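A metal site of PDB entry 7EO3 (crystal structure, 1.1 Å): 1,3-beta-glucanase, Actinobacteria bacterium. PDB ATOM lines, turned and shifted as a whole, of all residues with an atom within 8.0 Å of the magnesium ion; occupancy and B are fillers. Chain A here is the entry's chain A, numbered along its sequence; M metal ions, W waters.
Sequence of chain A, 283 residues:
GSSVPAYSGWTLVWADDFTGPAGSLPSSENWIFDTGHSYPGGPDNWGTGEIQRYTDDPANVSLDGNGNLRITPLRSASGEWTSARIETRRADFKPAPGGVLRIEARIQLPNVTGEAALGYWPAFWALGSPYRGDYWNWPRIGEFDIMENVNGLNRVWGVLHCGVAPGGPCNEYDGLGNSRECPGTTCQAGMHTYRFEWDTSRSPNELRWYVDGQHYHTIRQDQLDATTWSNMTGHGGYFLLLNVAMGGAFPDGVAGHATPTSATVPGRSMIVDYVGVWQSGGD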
ATOM      1  N   SER A   2       6.689  -9.758  -2.672  1.00  0.00           N
ATOM      2  CA  SER A   2       7.692 -10.671  -3.219  1.00  0.00           C
ATOM      3  C   SER A   2       7.102 -11.540  -4.325  1.00  0.00           C
ATOM      4  O   SER A   2       5.926 -11.930  -4.285  1.00  0.00           O
ATOM      5  CB  SER A   2       8.299 -11.524  -2.104  1.00  0.00           C
ATOM      6  OG  SER A   2       7.697 -12.803  -2.030  1.00  0.00           O
ATOM      7  N   SER A   3       7.936 -11.829  -5.336  1.00  0.00           N
ATOM      8  CA  SER A   3       7.654 -12.699  -6.477  1.00  0.00           C
ATOM      9  C   SER A   3       6.824 -12.018  -7.565  1.00  0.00           C
ATOM     10  O   SER A   3       6.177 -11.001  -7.317  1.00  0.00           O
ATOM     11  CB  SER A   3       7.053 -14.054  -6.056  1.00  0.00           C
ATOM     12  OG  SER A   3       5.648 -13.972  -5.915  1.00  0.00           O
ATOM     13  N   VAL A   4       6.861 -12.563  -8.774  1.00  0.00           N
ATOM     14  CA  VAL A   4       6.217 -11.934  -9.945  1.00  0.00           C
ATOM     15  C   VAL A   4       4.720 -11.818  -9.693  1.00  0.00           C
ATOM     16  O   VAL A   4       4.052 -12.834  -9.400  1.00  0.00           O
ATOM     17  CB  VAL A   4       6.489 -12.767 -11.210  1.00  0.00           C
ATOM     18  CG1 VAL A   4       5.683 -12.227 -12.370  1.00  0.00           C
ATOM     19  CG2 VAL A   4       7.968 -12.742 -11.560  1.00  0.00           C
ATOM     20  N   ASP A  16      11.555 -13.390 -15.320  1.00  0.00           N
ATOM     21  CA  ASP A  16      12.504 -14.202 -14.578  1.00  0.00           C
ATOM     22  C   ASP A  16      12.388 -13.824 -13.111  1.00  0.00           C
ATOM     23  O   ASP A  16      12.609 -12.663 -12.761  1.00  0.00           O
ATOM     24  CB  ASP A  16      13.928 -13.997 -15.106  1.00  0.00           C
ATOM     25  CG  ASP A  16      14.882 -15.082 -14.663  1.00  0.00           C
ATOM     26  OD1 ASP A  16      14.597 -15.755 -13.647  1.00  0.00           O
ATOM     27  OD2 ASP A  16      15.936 -15.269 -15.318  1.00  0.00           O
ATOM     28  N   ASP A  17      11.987 -14.781 -12.280  1.00  0.00           N
ATOM     29  CA  ASP A  17      11.885 -14.575 -10.838  1.00  0.00           C
ATOM     30  C   ASP A  17      13.145 -14.983 -10.103  1.00  0.00           C
ATOM     31  O   ASP A  17      13.191 -14.906  -8.871  1.00  0.00           O
ATOM     32  CB  ASP A  17      10.676 -15.337 -10.269  1.00  0.00           C
ATOM     33  CG  ASP A  17       9.938 -14.549  -9.171  1.00  0.00           C
ATOM     34  OD1 ASP A  17      10.537 -13.690  -8.486  1.00  0.00           O
ATOM     35  OD2 ASP A  17       8.729 -14.823  -8.990  1.00  0.00           O
ATOM     36  N   PHE A  18      14.184 -15.424 -10.832  1.00  0.00           N
ATOM     37  CA  PHE A  18      15.495 -15.688 -10.250  1.00  0.00           C
ATOM     38  C   PHE A  18      15.468 -16.735  -9.146  1.00  0.00           C
ATOM     39  O   PHE A  18      16.191 -16.660  -8.155  1.00  0.00           O
ATOM     40  CB  PHE A  18      16.191 -14.392  -9.813  1.00  0.00           C
ATOM     41  CG  PHE A  18      16.426 -13.440 -10.946  1.00  0.00           C
ATOM     42  CD1 PHE A  18      17.240 -13.801 -12.003  1.00  0.00           C
ATOM     43  CD2 PHE A  18      15.820 -12.186 -10.969  1.00  0.00           C
ATOM     44  CE1 PHE A  18      17.472 -12.931 -13.058  1.00  0.00           C
ATOM     45  CE2 PHE A  18      16.052 -11.316 -12.024  1.00  0.00           C
ATOM     46  CZ  PHE A  18      16.880 -11.687 -13.064  1.00  0.00           C
ATOM     47  N   THR A  19      14.670 -17.770  -9.353  1.00  0.00           N
ATOM     48  CA  THR A  19      14.640 -18.887  -8.425  1.00  0.00           C
ATOM     49  C   THR A  19      15.714 -19.888  -8.810  1.00  0.00           C
ATOM     50  O   THR A  19      16.052 -20.076  -9.985  1.00  0.00           O
ATOM     51  CB  THR A  19      13.263 -19.540  -8.402  1.00  0.00           C
ATOM     52  OG1 THR A  19      13.003 -20.126  -9.681  1.00  0.00           O
ATOM     53  CG2 THR A  19      12.191 -18.517  -8.094  1.00  0.00           C
ATOM     54  N   GLY A  20      16.295 -20.522  -7.790  1.00  0.00           N
ATOM     55  CA  GLY A  20      17.354 -21.474  -8.008  1.00  0.00           C
ATOM     56  C   GLY A  20      18.387 -21.384  -6.914  1.00  0.00           C
ATOM     57  O   GLY A  20      18.340 -20.500  -6.061  1.00  0.00           O
ATOM     58  N   ASP A  64      20.800 -15.901  -5.114  1.00  0.00           N
ATOM     59  CA  ASP A  64      21.040 -15.988  -3.686  1.00  0.00           C
ATOM     60  C   ASP A  64      20.373 -17.191  -3.026  1.00  0.00           C
ATOM     61  O   ASP A  64      20.564 -17.412  -1.829  1.00  0.00           O
ATOM     62  CB  ASP A  64      20.697 -14.674  -2.967  1.00  0.00           C
ATOM     63  CG  ASP A  64      19.192 -14.422  -2.867  1.00  0.00           C
ATOM     64  OD1 ASP A  64      18.386 -15.155  -3.458  1.00  0.00           O
ATOM     65  OD2 ASP A  64      18.809 -13.444  -2.190  1.00  0.00           O
ATOM     66  N   ASN A  66      17.281 -17.442  -2.504  1.00  0.00           N
ATOM     67  CA  ASN A  66      16.048 -16.932  -1.917  1.00  0.00           C
ATOM     68  C   ASN A  66      15.134 -16.304  -2.944  1.00  0.00           C
ATOM     69  O   ASN A  66      14.200 -15.587  -2.569  1.00  0.00           O
ATOM     70  CB  ASN A  66      16.351 -15.895  -0.832  1.00  0.00           C
ATOM     71  CG  ASN A  66      17.344 -16.376   0.202  1.00  0.00           C
ATOM     72  OD1 ASN A  66      17.252 -17.506   0.682  1.00  0.00           O
ATOM     73  ND2 ASN A  66      18.300 -15.522   0.559  1.00  0.00           N
ATOM     74  N   GLY A  67      15.395 -16.522  -4.233  1.00  0.00           N
ATOM     75  CA  GLY A  67      14.577 -15.934  -5.275  1.00  0.00           C
ATOM     76  C   GLY A  67      15.062 -14.597  -5.800  1.00  0.00           C
ATOM     77  O   GLY A  67      14.283 -13.890  -6.448  1.00  0.00           O
ATOM     78  N   ASN A  68      16.313 -14.219  -5.538  1.00  0.00           N
ATOM     79  CA  ASN A  68      16.867 -12.980  -6.051  1.00  0.00           C
ATOM     80  C   ASN A  68      18.156 -13.219  -6.794  1.00  0.00           C
ATOM     81  O   ASN A  68      18.936 -14.134  -6.489  1.00  0.00           O
ATOM     82  CB  ASN A  68      17.195 -11.994  -4.924  1.00  0.00           C
ATOM     83  CG  ASN A  68      16.053 -11.822  -3.951  1.00  0.00           C
ATOM     84  OD1 ASN A  68      14.998 -11.308  -4.309  1.00  0.00           O
ATOM     85  ND2 ASN A  68      16.269 -12.241  -2.721  1.00  0.00           N
ATOM     86  N   LEU A  69      18.406 -12.342  -7.767  1.00  0.00           N
ATOM     87  CA  LEU A  69      19.704 -12.210  -8.394  1.00  0.00           C
ATOM     88  C   LEU A  69      20.512 -11.173  -7.610  1.00  0.00           C
ATOM     89  O   LEU A  69      19.966 -10.154  -7.186  1.00  0.00           O
ATOM     90  CB  LEU A  69      19.516 -11.689  -9.815  1.00  0.00           C
ATOM     91  CG  LEU A  69      20.799 -11.416 -10.589  1.00  0.00           C
ATOM     92  CD1 LEU A  69      21.502 -12.727 -10.926  1.00  0.00           C
ATOM     93  CD2 LEU A  69      20.488 -10.634 -11.851  1.00  0.00           C
ATOM     94  N   ARG A 106      11.627  -5.567  -9.499  1.00  0.00           N
ATOM     95  CA  ARG A 106      11.644  -5.312  -8.068  1.00  0.00           C
ATOM     96  C   ARG A 106      13.087  -5.451  -7.603  1.00  0.00           C
ATOM     97  O   ARG A 106      13.673  -6.529  -7.731  1.00  0.00           O
ATOM     98  CB  ARG A 106      10.735  -6.304  -7.344  1.00  0.00           C
ATOM     99  CG  ARG A 106      10.602  -6.040  -5.858  1.00  0.00           C
ATOM    100  CD  ARG A 106       9.535  -6.923  -5.259  1.00  0.00           C
ATOM    101  NE  ARG A 106       9.324  -6.623  -3.850  1.00  0.00           N
ATOM    102  CZ  ARG A 106       9.813  -7.357  -2.850  1.00  0.00           C
ATOM    103  NH1 ARG A 106      10.539  -8.440  -3.111  1.00  0.00           N
ATOM    104  NH2 ARG A 106       9.571  -6.987  -1.601  1.00  0.00           N
ATOM    105  N   MET A 191      13.521  -3.182  -0.907  1.00  0.00           N
ATOM    106  CA  MET A 191      13.026  -3.482  -2.236  1.00  0.00           C
ATOM    107  C   MET A 191      11.981  -2.459  -2.671  1.00  0.00           C
ATOM    108  O   MET A 191      11.091  -2.085  -1.891  1.00  0.00           O
ATOM    109  CB  MET A 191      12.352  -4.856  -2.231  1.00  0.00           C
ATOM    110  CG  MET A 191      13.312  -6.017  -2.254  1.00  0.00           C
ATOM    111  SD  MET A 191      13.898  -6.287  -3.925  1.00  0.00           S
ATOM    112  CE  MET A 191      15.122  -7.556  -3.663  1.00  0.00           C
ATOM    113  N   VAL A 272      17.860  -8.286  -7.095  1.00  0.00           N
ATOM    114  CA  VAL A 272      16.716  -8.222  -7.994  1.00  0.00           C
ATOM    115  C   VAL A 272      15.813  -9.422  -7.736  1.00  0.00           C
ATOM    116  O   VAL A 272      16.214 -10.568  -7.987  1.00  0.00           O
ATOM    117  CB  VAL A 272      17.148  -8.188  -9.471  1.00  0.00           C
ATOM    118  CG1 VAL A 272      15.936  -7.974 -10.368  1.00  0.00           C
ATOM    119  CG2 VAL A 272      18.208  -7.105  -9.698  1.00  0.00           C
ATOM    120  N   ASP A 273      14.588  -9.176  -7.272  1.00  0.00           N
ATOM    121  CA  ASP A 273      13.638 -10.265  -7.053  1.00  0.00           C
ATOM    122  C   ASP A 273      13.118 -10.814  -8.380  1.00  0.00           C
ATOM    123  O   ASP A 273      13.020 -12.034  -8.558  1.00  0.00           O
ATOM    124  CB  ASP A 273      12.497  -9.784  -6.161  1.00  0.00           C
ATOM    125  CG  ASP A 273      11.472 -10.857  -5.851  1.00  0.00           C
ATOM    126  OD1 ASP A 273      11.701 -12.052  -6.117  1.00  0.00           O
ATOM    127  OD2 ASP A 273      10.428 -10.478  -5.285  1.00  0.00           O
ATOM    128  N   TYR A 274      12.756  -9.927  -9.309  1.00  0.00           N
ATOM    129  CA  TYR A 274      12.235 -10.373 -10.594  1.00  0.00           C
ATOM    130  C   TYR A 274      12.318  -9.243 -11.594  1.00  0.00           C
ATOM    131  O   TYR A 274      12.438  -8.066 -11.231  1.00  0.00           O
ATOM    132  CB  TYR A 274      10.773 -10.866 -10.489  1.00  0.00           C
ATOM    133  CG  TYR A 274       9.747  -9.757 -10.261  1.00  0.00           C
ATOM    134  CD1 TYR A 274       9.239  -8.993 -11.315  1.00  0.00           C
ATOM    135  CD2 TYR A 274       9.272  -9.482  -8.981  1.00  0.00           C
ATOM    136  CE1 TYR A 274       8.310  -7.989 -11.115  1.00  0.00           C
ATOM    137  CE2 TYR A 274       8.345  -8.470  -8.761  1.00  0.00           C
ATOM    138  CZ  TYR A 274       7.869  -7.726  -9.830  1.00  0.00           C
ATOM    139  OH  TYR A 274       6.945  -6.721  -9.622  1.00  0.00           O
ATOM    140  N   VAL A 275      12.281  -9.641 -12.867  1.00  0.00           N
ATOM    141  CA  VAL A 275      12.020  -8.778 -14.008  1.00  0.00           C
ATOM    142  C   VAL A 275      10.850  -9.388 -14.766  1.00  0.00           C
ATOM    143  O   VAL A 275      10.793 -10.604 -14.946  1.00  0.00           O
ATOM    144  CB  VAL A 275      13.249  -8.712 -14.949  1.00  0.00           C
ATOM    145  CG1 VAL A 275      12.972  -7.789 -16.127  1.00  0.00           C
ATOM    146  CG2 VAL A 275      14.500  -8.278 -14.209  1.00  0.00           C
HETATM  147 MG    MG M   1      12.331 -13.693  -7.311  1.00  0.00          MG
HETATM  148  O   HOH W   1      11.507 -15.224  -6.303  1.00  0.00           O
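The magnesium ion is bound by water W1 (2.0 Å), OD1 of Asp 273 (2.1 Å), O of Gly 67 (2.1 Å), OD1 of Asp 17 (2.1 Å), O of Asp 17 (2.2 Å) and O of Asp 273 (2.2 Å).
The nearest printed residue that does not touch the magnesium ion is Tyr 274 (4.3 Å).
The side-chain carboxylate (OD2) of Asp 273 lies within hydrogen-bond range of the backbone NH (N) of Ser 3.
OD2 of Asp 273 is in salt-bridge range of NH1 of Arg 106.
OD2 of Asp 17 lies within hydrogen-bond range of N of Val 4 (2.9 Å).
OD1 of Asp 64 sits at hydrogen-bond distance from N of Gly 67 (3.4 Å).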
